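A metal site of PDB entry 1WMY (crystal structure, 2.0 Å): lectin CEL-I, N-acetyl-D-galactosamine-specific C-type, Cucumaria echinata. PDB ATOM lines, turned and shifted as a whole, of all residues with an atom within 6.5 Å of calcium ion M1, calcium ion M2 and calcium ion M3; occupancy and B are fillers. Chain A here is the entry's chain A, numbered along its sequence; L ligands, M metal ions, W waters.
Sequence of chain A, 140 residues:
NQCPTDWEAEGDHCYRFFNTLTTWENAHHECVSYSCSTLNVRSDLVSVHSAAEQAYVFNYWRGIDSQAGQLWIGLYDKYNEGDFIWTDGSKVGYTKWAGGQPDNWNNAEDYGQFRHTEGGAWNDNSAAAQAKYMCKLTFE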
ATOM      1  N   ASP A  77     -10.316  -9.608  -5.022  1.00  0.00           N
ATOM      2  CA  ASP A  77     -10.162  -8.240  -4.532  1.00  0.00           C
ATOM      3  C   ASP A  77      -8.862  -7.559  -5.037  1.00  0.00           C
ATOM      4  O   ASP A  77      -8.212  -6.768  -4.305  1.00  0.00           O
ATOM      5  CB  ASP A  77     -10.238  -8.208  -3.016  1.00  0.00           C
ATOM      6  CG  ASP A  77      -8.972  -8.707  -2.347  1.00  0.00           C
ATOM      7  OD1 ASP A  77      -8.223  -9.516  -2.912  1.00  0.00           O
ATOM      8  OD2 ASP A  77      -8.654  -8.350  -1.191  1.00  0.00           O
ATOM      9  N   LYS A  78      -8.540  -7.847  -6.267  1.00  0.00           N
ATOM     10  CA  LYS A  78      -7.453  -7.210  -6.974  1.00  0.00           C
ATOM     11  C   LYS A  78      -7.602  -5.695  -7.055  1.00  0.00           C
ATOM     12  O   LYS A  78      -6.596  -4.971  -6.891  1.00  0.00           O
ATOM     13  CB  LYS A  78      -7.347  -7.878  -8.377  1.00  0.00           C
ATOM     14  CG  LYS A  78      -6.212  -7.496  -9.271  1.00  0.00           C
ATOM     15  CD  LYS A  78      -5.759  -8.684 -10.233  1.00  0.00           C
ATOM     16  CE  LYS A  78      -6.931  -9.162 -11.174  1.00  0.00           C
ATOM     17  NZ  LYS A  78      -6.593 -10.226 -12.255  1.00  0.00           N
ATOM     18  N   ASN A  80      -9.686  -3.555  -5.347  1.00  0.00           N
ATOM     19  CA  ASN A  80      -9.906  -2.930  -4.073  1.00  0.00           C
ATOM     20  C   ASN A  80      -9.666  -3.973  -2.977  1.00  0.00           C
ATOM     21  O   ASN A  80     -10.548  -4.716  -2.614  1.00  0.00           O
ATOM     22  CB  ASN A  80     -11.339  -2.409  -4.027  1.00  0.00           C
ATOM     23  CG  ASN A  80     -11.560  -1.180  -4.891  1.00  0.00           C
ATOM     24  OD1 ASN A  80     -11.360  -0.052  -4.438  1.00  0.00           O
ATOM     25  ND2 ASN A  80     -11.863  -1.404  -6.159  1.00  0.00           N
ATOM     26  N   GLU A  81      -8.484  -3.947  -2.380  1.00  0.00           N
ATOM     27  CA  GLU A  81      -8.071  -4.907  -1.421  1.00  0.00           C
ATOM     28  C   GLU A  81      -9.067  -4.930  -0.274  1.00  0.00           C
ATOM     29  O   GLU A  81      -9.412  -3.860   0.186  1.00  0.00           O
ATOM     30  CB  GLU A  81      -6.644  -4.559  -0.932  1.00  0.00           C
ATOM     31  CG  GLU A  81      -6.175  -5.456   0.234  1.00  0.00           C
ATOM     32  CD  GLU A  81      -6.132  -6.939  -0.143  1.00  0.00           C
ATOM     33  OE1 GLU A  81      -6.590  -7.809   0.638  1.00  0.00           O
ATOM     34  OE2 GLU A  81      -5.649  -7.281  -1.217  1.00  0.00           O
ATOM     35  N   GLY A  82      -9.521  -6.103   0.136  1.00  0.00           N
ATOM     36  CA  GLY A  82     -10.482  -6.308   1.230  1.00  0.00           C
ATOM     37  C   GLY A  82     -11.951  -6.204   0.809  1.00  0.00           C
ATOM     38  O   GLY A  82     -12.796  -6.520   1.578  1.00  0.00           O
ATOM     39  N   PHE A  84     -14.088  -7.719  -1.838  1.00  0.00           N
ATOM     40  CA  PHE A  84     -14.222  -8.763  -2.849  1.00  0.00           C
ATOM     41  C   PHE A  84     -15.465  -8.519  -3.713  1.00  0.00           C
ATOM     42  O   PHE A  84     -16.531  -8.090  -3.191  1.00  0.00           O
ATOM     43  CB  PHE A  84     -14.293 -10.100  -2.154  1.00  0.00           C
ATOM     44  CG  PHE A  84     -12.966 -10.575  -1.653  1.00  0.00           C
ATOM     45  CD1 PHE A  84     -12.185 -11.363  -2.448  1.00  0.00           C
ATOM     46  CD2 PHE A  84     -12.514 -10.205  -0.402  1.00  0.00           C
ATOM     47  CE1 PHE A  84     -10.944 -11.828  -2.005  1.00  0.00           C
ATOM     48  CE2 PHE A  84     -11.282 -10.623   0.053  1.00  0.00           C
ATOM     49  CZ  PHE A  84     -10.501 -11.460  -0.751  1.00  0.00           C
ATOM     50  N   GLY A 100     -10.779 -16.960  10.119  1.00  0.00           N
ATOM     51  CA  GLY A 100      -9.506 -16.332   9.903  1.00  0.00           C
ATOM     52  C   GLY A 100      -9.291 -15.877   8.476  1.00  0.00           C
ATOM     53  O   GLY A 100      -8.183 -15.505   8.086  1.00  0.00           O
ATOM     54  N   GLN A 101     -10.364 -15.962   7.687  1.00  0.00           N
ATOM     55  CA  GLN A 101     -10.329 -15.504   6.277  1.00  0.00           C
ATOM     56  C   GLN A 101     -11.355 -14.377   6.016  1.00  0.00           C
ATOM     57  O   GLN A 101     -12.363 -14.322   6.666  1.00  0.00           O
ATOM     58  CB  GLN A 101     -10.597 -16.683   5.377  1.00  0.00           C
ATOM     59  CG  GLN A 101      -9.715 -17.922   5.594  1.00  0.00           C
ATOM     60  CD  GLN A 101      -8.266 -17.646   5.417  1.00  0.00           C
ATOM     61  OE1 GLN A 101      -7.894 -16.781   4.597  1.00  0.00           O
ATOM     62  NE2 GLN A 101      -7.403 -18.356   6.201  1.00  0.00           N
ATOM     63  N   PRO A 102     -11.134 -13.523   5.013  1.00  0.00           N
ATOM     64  CA  PRO A 102      -9.970 -13.524   4.142  1.00  0.00           C
ATOM     65  C   PRO A 102      -8.804 -12.777   4.819  1.00  0.00           C
ATOM     66  O   PRO A 102      -9.053 -11.704   5.386  1.00  0.00           O
ATOM     67  CB  PRO A 102     -10.482 -12.794   2.896  1.00  0.00           C
ATOM     68  CG  PRO A 102     -11.510 -11.827   3.365  1.00  0.00           C
ATOM     69  CD  PRO A 102     -12.110 -12.471   4.633  1.00  0.00           C
ATOM     70  N   ASP A 103      -7.597 -13.325   4.791  1.00  0.00           N
ATOM     71  CA  ASP A 103      -6.469 -12.728   5.559  1.00  0.00           C
ATOM     72  C   ASP A 103      -5.394 -12.110   4.650  1.00  0.00           C
ATOM     73  O   ASP A 103      -4.476 -11.467   5.127  1.00  0.00           O
ATOM     74  CB  ASP A 103      -5.850 -13.738   6.473  1.00  0.00           C
ATOM     75  CG  ASP A 103      -5.243 -14.941   5.684  1.00  0.00           C
ATOM     76  OD1 ASP A 103      -4.611 -15.831   6.291  1.00  0.00           O
ATOM     77  OD2 ASP A 103      -5.348 -15.024   4.449  1.00  0.00           O
ATOM     78  N   ASN A 104      -5.547 -12.190   3.331  1.00  0.00           N
ATOM     79  CA  ASN A 104      -4.583 -11.544   2.405  1.00  0.00           C
ATOM     80  C   ASN A 104      -3.147 -11.956   2.756  1.00  0.00           C
ATOM     81  O   ASN A 104      -2.229 -11.087   2.910  1.00  0.00           O
ATOM     82  CB  ASN A 104      -4.679  -9.998   2.457  1.00  0.00           C
ATOM     83  CG  ASN A 104      -4.080  -9.358   1.179  1.00  0.00           C
ATOM     84  OD1 ASN A 104      -4.242  -9.871   0.107  1.00  0.00           O
ATOM     85  ND2 ASN A 104      -3.337  -8.244   1.345  1.00  0.00           N
ATOM     86  N   TRP A 105      -2.981 -13.245   3.028  1.00  0.00           N
ATOM     87  CA  TRP A 105      -1.701 -13.749   3.562  1.00  0.00           C
ATOM     88  C   TRP A 105      -0.493 -13.321   2.734  1.00  0.00           C
ATOM     89  O   TRP A 105      -0.511 -13.368   1.500  1.00  0.00           O
ATOM     90  CB  TRP A 105      -1.746 -15.286   3.698  1.00  0.00           C
ATOM     91  CG  TRP A 105      -0.531 -15.812   4.243  1.00  0.00           C
ATOM     92  CD1 TRP A 105      -0.147 -15.793   5.552  1.00  0.00           C
ATOM     93  CD2 TRP A 105       0.568 -16.347   3.519  1.00  0.00           C
ATOM     94  NE1 TRP A 105       1.091 -16.338   5.697  1.00  0.00           N
ATOM     95  CE2 TRP A 105       1.578 -16.675   4.463  1.00  0.00           C
ATOM     96  CE3 TRP A 105       0.818 -16.588   2.165  1.00  0.00           C
ATOM     97  CZ2 TRP A 105       2.786 -17.280   4.103  1.00  0.00           C
ATOM     98  CZ3 TRP A 105       2.059 -17.157   1.804  1.00  0.00           C
ATOM     99  CH2 TRP A 105       3.020 -17.485   2.768  1.00  0.00           C
ATOM    100  N   ASN A 107       0.461 -10.413   2.161  1.00  0.00           N
ATOM    101  CA  ASN A 107      -0.008  -9.300   1.374  1.00  0.00           C
ATOM    102  C   ASN A 107      -0.232  -9.682  -0.101  1.00  0.00           C
ATOM    103  O   ASN A 107      -0.128  -8.847  -1.007  1.00  0.00           O
ATOM    104  CB  ASN A 107       0.927  -8.045   1.551  1.00  0.00           C
ATOM    105  CG  ASN A 107       0.176  -6.678   1.205  1.00  0.00           C
ATOM    106  OD1 ASN A 107      -1.083  -6.623   1.211  1.00  0.00           O
ATOM    107  ND2 ASN A 107       0.942  -5.611   0.872  1.00  0.00           N
ATOM    108  N   ALA A 108      -0.581 -10.951  -0.359  1.00  0.00           N
ATOM    109  CA  ALA A 108      -0.611 -11.451  -1.696  1.00  0.00           C
ATOM    110  C   ALA A 108      -1.700 -12.444  -2.064  1.00  0.00           C
ATOM    111  O   ALA A 108      -1.445 -13.292  -2.933  1.00  0.00           O
ATOM    112  CB  ALA A 108       0.771 -12.103  -2.063  1.00  0.00           C
ATOM    113  N   GLU A 109      -2.861 -12.367  -1.433  1.00  0.00           N
ATOM    114  CA  GLU A 109      -3.972 -13.235  -1.757  1.00  0.00           C
ATOM    115  C   GLU A 109      -5.224 -12.474  -2.174  1.00  0.00           C
ATOM    116  O   GLU A 109      -5.920 -11.900  -1.335  1.00  0.00           O
ATOM    117  CB  GLU A 109      -4.296 -14.146  -0.540  1.00  0.00           C
ATOM    118  CG  GLU A 109      -3.086 -14.995  -0.096  1.00  0.00           C
ATOM    119  CD  GLU A 109      -3.488 -16.082   0.915  1.00  0.00           C
ATOM    120  OE1 GLU A 109      -4.312 -15.787   1.822  1.00  0.00           O
ATOM    121  OE2 GLU A 109      -3.047 -17.254   0.780  1.00  0.00           O
ATOM    122  N   ASP A 110      -5.522 -12.494  -3.486  1.00  0.00           N
ATOM    123  CA  ASP A 110      -6.653 -11.751  -3.982  1.00  0.00           C
ATOM    124  C   ASP A 110      -7.774 -12.626  -4.593  1.00  0.00           C
ATOM    125  O   ASP A 110      -8.632 -12.127  -5.275  1.00  0.00           O
ATOM    126  CB  ASP A 110      -6.174 -10.661  -4.952  1.00  0.00           C
ATOM    127  CG  ASP A 110      -5.366  -9.573  -4.245  1.00  0.00           C
ATOM    128  OD1 ASP A 110      -4.829  -8.740  -4.943  1.00  0.00           O
ATOM    129  OD2 ASP A 110      -5.305  -9.449  -2.977  1.00  0.00           O
ATOM    130  N   TYR A 111      -7.718 -13.922  -4.366  1.00  0.00           N
ATOM    131  CA  TYR A 111      -8.503 -14.814  -5.206  1.00  0.00           C
ATOM    132  C   TYR A 111      -9.203 -15.854  -4.347  1.00  0.00           C
ATOM    133  O   TYR A 111      -8.575 -16.600  -3.585  1.00  0.00           O
ATOM    134  CB  TYR A 111      -7.639 -15.549  -6.210  1.00  0.00           C
ATOM    135  CG  TYR A 111      -6.807 -14.628  -7.068  1.00  0.00           C
ATOM    136  CD1 TYR A 111      -5.441 -14.646  -7.009  1.00  0.00           C
ATOM    137  CD2 TYR A 111      -7.430 -13.773  -7.962  1.00  0.00           C
ATOM    138  CE1 TYR A 111      -4.698 -13.803  -7.802  1.00  0.00           C
ATOM    139  CE2 TYR A 111      -6.750 -12.912  -8.732  1.00  0.00           C
ATOM    140  CZ  TYR A 111      -5.372 -12.924  -8.700  1.00  0.00           C
ATOM    141  OH  TYR A 111      -4.664 -12.061  -9.520  1.00  0.00           O
ATOM    142  N   ARG A 115     -12.594 -24.348   0.172  1.00  0.00           N
ATOM    143  CA  ARG A 115     -11.875 -25.512   0.672  1.00  0.00           C
ATOM    144  C   ARG A 115     -12.747 -26.770   0.486  1.00  0.00           C
ATOM    145  O   ARG A 115     -13.980 -26.658   0.381  1.00  0.00           O
ATOM    146  CB  ARG A 115     -11.615 -25.321   2.155  1.00  0.00           C
ATOM    147  CG  ARG A 115     -10.632 -24.196   2.443  1.00  0.00           C
ATOM    148  CD  ARG A 115     -10.370 -24.184   3.911  1.00  0.00           C
ATOM    149  NE  ARG A 115      -9.511 -23.083   4.265  1.00  0.00           N
ATOM    150  CZ  ARG A 115      -9.283 -22.676   5.491  1.00  0.00           C
ATOM    151  NH1 ARG A 115      -9.855 -23.305   6.545  1.00  0.00           N
ATOM    152  NH2 ARG A 115      -8.468 -21.626   5.653  1.00  0.00           N
ATOM    153  N   ASN A 123     -11.638 -19.510   1.282  1.00  0.00           N
ATOM    154  CA  ASN A 123     -10.340 -18.960   1.605  1.00  0.00           C
ATOM    155  C   ASN A 123      -9.927 -18.035   0.445  1.00  0.00           C
ATOM    156  O   ASN A 123     -10.381 -18.197  -0.693  1.00  0.00           O
ATOM    157  CB  ASN A 123      -9.359 -20.104   1.702  1.00  0.00           C
ATOM    158  CG  ASN A 123      -7.936 -19.621   1.879  1.00  0.00           C
ATOM    159  OD1 ASN A 123      -7.681 -18.778   2.709  1.00  0.00           O
ATOM    160  ND2 ASN A 123      -7.017 -20.191   1.135  1.00  0.00           N
ATOM    161  N   ASP A 124      -9.113 -17.019   0.747  1.00  0.00           N
ATOM    162  CA  ASP A 124      -8.442 -16.260  -0.286  1.00  0.00           C
ATOM    163  C   ASP A 124      -7.044 -16.839  -0.466  1.00  0.00           C
ATOM    164  O   ASP A 124      -6.364 -17.166   0.500  1.00  0.00           O
ATOM    165  CB  ASP A 124      -8.383 -14.787   0.023  1.00  0.00           C
ATOM    166  CG  ASP A 124      -7.671 -14.453   1.348  1.00  0.00           C
ATOM    167  OD1 ASP A 124      -7.508 -15.344   2.192  1.00  0.00           O
ATOM    168  OD2 ASP A 124      -7.283 -13.286   1.571  1.00  0.00           O
ATOM    169  N   ASN A 125      -6.601 -16.890  -1.719  1.00  0.00           N
ATOM    170  CA  ASN A 125      -5.322 -17.453  -2.022  1.00  0.00           C
ATOM    171  C   ASN A 125      -4.647 -16.632  -3.131  1.00  0.00           C
ATOM    172  O   ASN A 125      -5.174 -15.636  -3.615  1.00  0.00           O
ATOM    173  CB  ASN A 125      -5.515 -18.920  -2.379  1.00  0.00           C
ATOM    174  CG  ASN A 125      -4.315 -19.801  -2.030  1.00  0.00           C
ATOM    175  OD1 ASN A 125      -3.159 -19.412  -2.178  1.00  0.00           O
ATOM    176  ND2 ASN A 125      -4.620 -21.032  -1.684  1.00  0.00           N
HETATM  177  C1  LIG L   1      -2.195 -19.703   2.545  1.00  0.00           C
HETATM  178  C2  LIG L   1      -3.664 -19.950   2.756  1.00  0.00           C
HETATM  179  O1  LIG L   1      -4.439 -18.842   2.203  1.00  0.00           O
HETATM  180  C3  LIG L   1      -3.941 -21.261   2.023  1.00  0.00           C
HETATM  181  C4  LIG L   1      -4.006 -20.053   4.236  1.00  0.00           C
HETATM  182  C5  LIG L   1      -3.768 -18.772   4.991  1.00  0.00           C
HETATM  183  O2  LIG L   1      -4.906 -17.946   5.007  1.00  0.00           O
HETATM  184  C6  LIG L   1      -3.369 -19.023   6.417  1.00  0.00           C
HETATM  185 CA    CA M   1      -6.546  -9.588  -1.036  1.00  0.00          CA
HETATM  186 CA    CA M   2      -6.000 -16.957   2.979  1.00  0.00          CA
HETATM  187 CA    CA M   3      -4.243  -7.262  -3.083  1.00  0.00          CA
HETATM  188  O   HOH W   1      -2.702  -8.619  -1.988  1.00  0.00           O
HETATM  189  O   HOH W   2      -5.754  -5.790  -3.902  1.00  0.00           O
HETATM  190  O   HOH W   3      -2.697  -6.313  -4.660  1.00  0.00           O
HETATM  191  O   HOH W   4      -7.570 -10.743   0.924  1.00  0.00           O
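Calcium ion M2 is bound by the side-chain carboxylate (OD1) of Asp 124 (2.3 Å), the side-chain carboxylate (OE1) of Glu 109 (2.4 Å), the side-chain amide oxygen (OD1) of Asn 123 (2.5 Å), the side-chain amide oxygen (OE1) of Gln 101 (2.5 Å), an oxygen (O2) of the ligand (2.5 Å), the side-chain carboxylate (OD2) of Asp 103 (2.5 Å), the backbone carbonyl oxygen (O) of Asp 124 (2.5 Å) and an oxygen (O1) of the ligand (2.6 Å).
Calcium ion M3 is bound by water W2, water W1, OE2 of Glu 81, water W3, OD2 of Asp 110 and OD1 of Asp 110.
Calcium ion M1 is bound by the side-chain carboxylate (OD2) of Asp 110, the backbone carbonyl oxygen (O) of Glu 109, the side-chain carboxylate (OE1) of Glu 81, the side-chain carboxylate (OD2) of Asp 77, the side-chain carboxylate (OE2) of Glu 81, water W4, the side-chain carboxylate (OD1) of Asp 77 and the side-chain amide oxygen (OD1) of Asn 104.
The side-chain carboxylate (OD2) of Asp 77 sits close to the backbone NH (N) of Gly 82 (2.7 Å). The side-chain amide nitrogen (ND2) of Asn 104 lies within hydrogen-bond range of the side-chain amide oxygen (OD1) of Asn 107 (2.8 Å). OE1 of Glu 109 sits close to N of Trp 105, 3.1 Å away. The backbone NH of Asp 110 lies within hydrogen-bond range of the backbone carbonyl oxygen of Asn 125 (3.2 Å). OD2 of Asp 124 sits at hydrogen-bond distance from N of Asn 104 (2.7 Å). The side-chain carboxylate of Asp 103 lies close to the backbone NH of Trp 105, at 3.3 Å. NH2 of Arg 115 lies close to NE2 of Gln 101, at 3.5 Å.
Water W4 bridges OD2 of Asp 124 (2.6 Å) and N of Asn 104 (3.5 Å). Water W1 lies within hydrogen-bond range of O of Asn 107 (2.8 Å) and ND2 of Asn 104 (3.4 Å).
Within 4 Å of calcium ion M1: Asp 77, Glu 81, Asn 104, Glu 109 and Asp 110.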
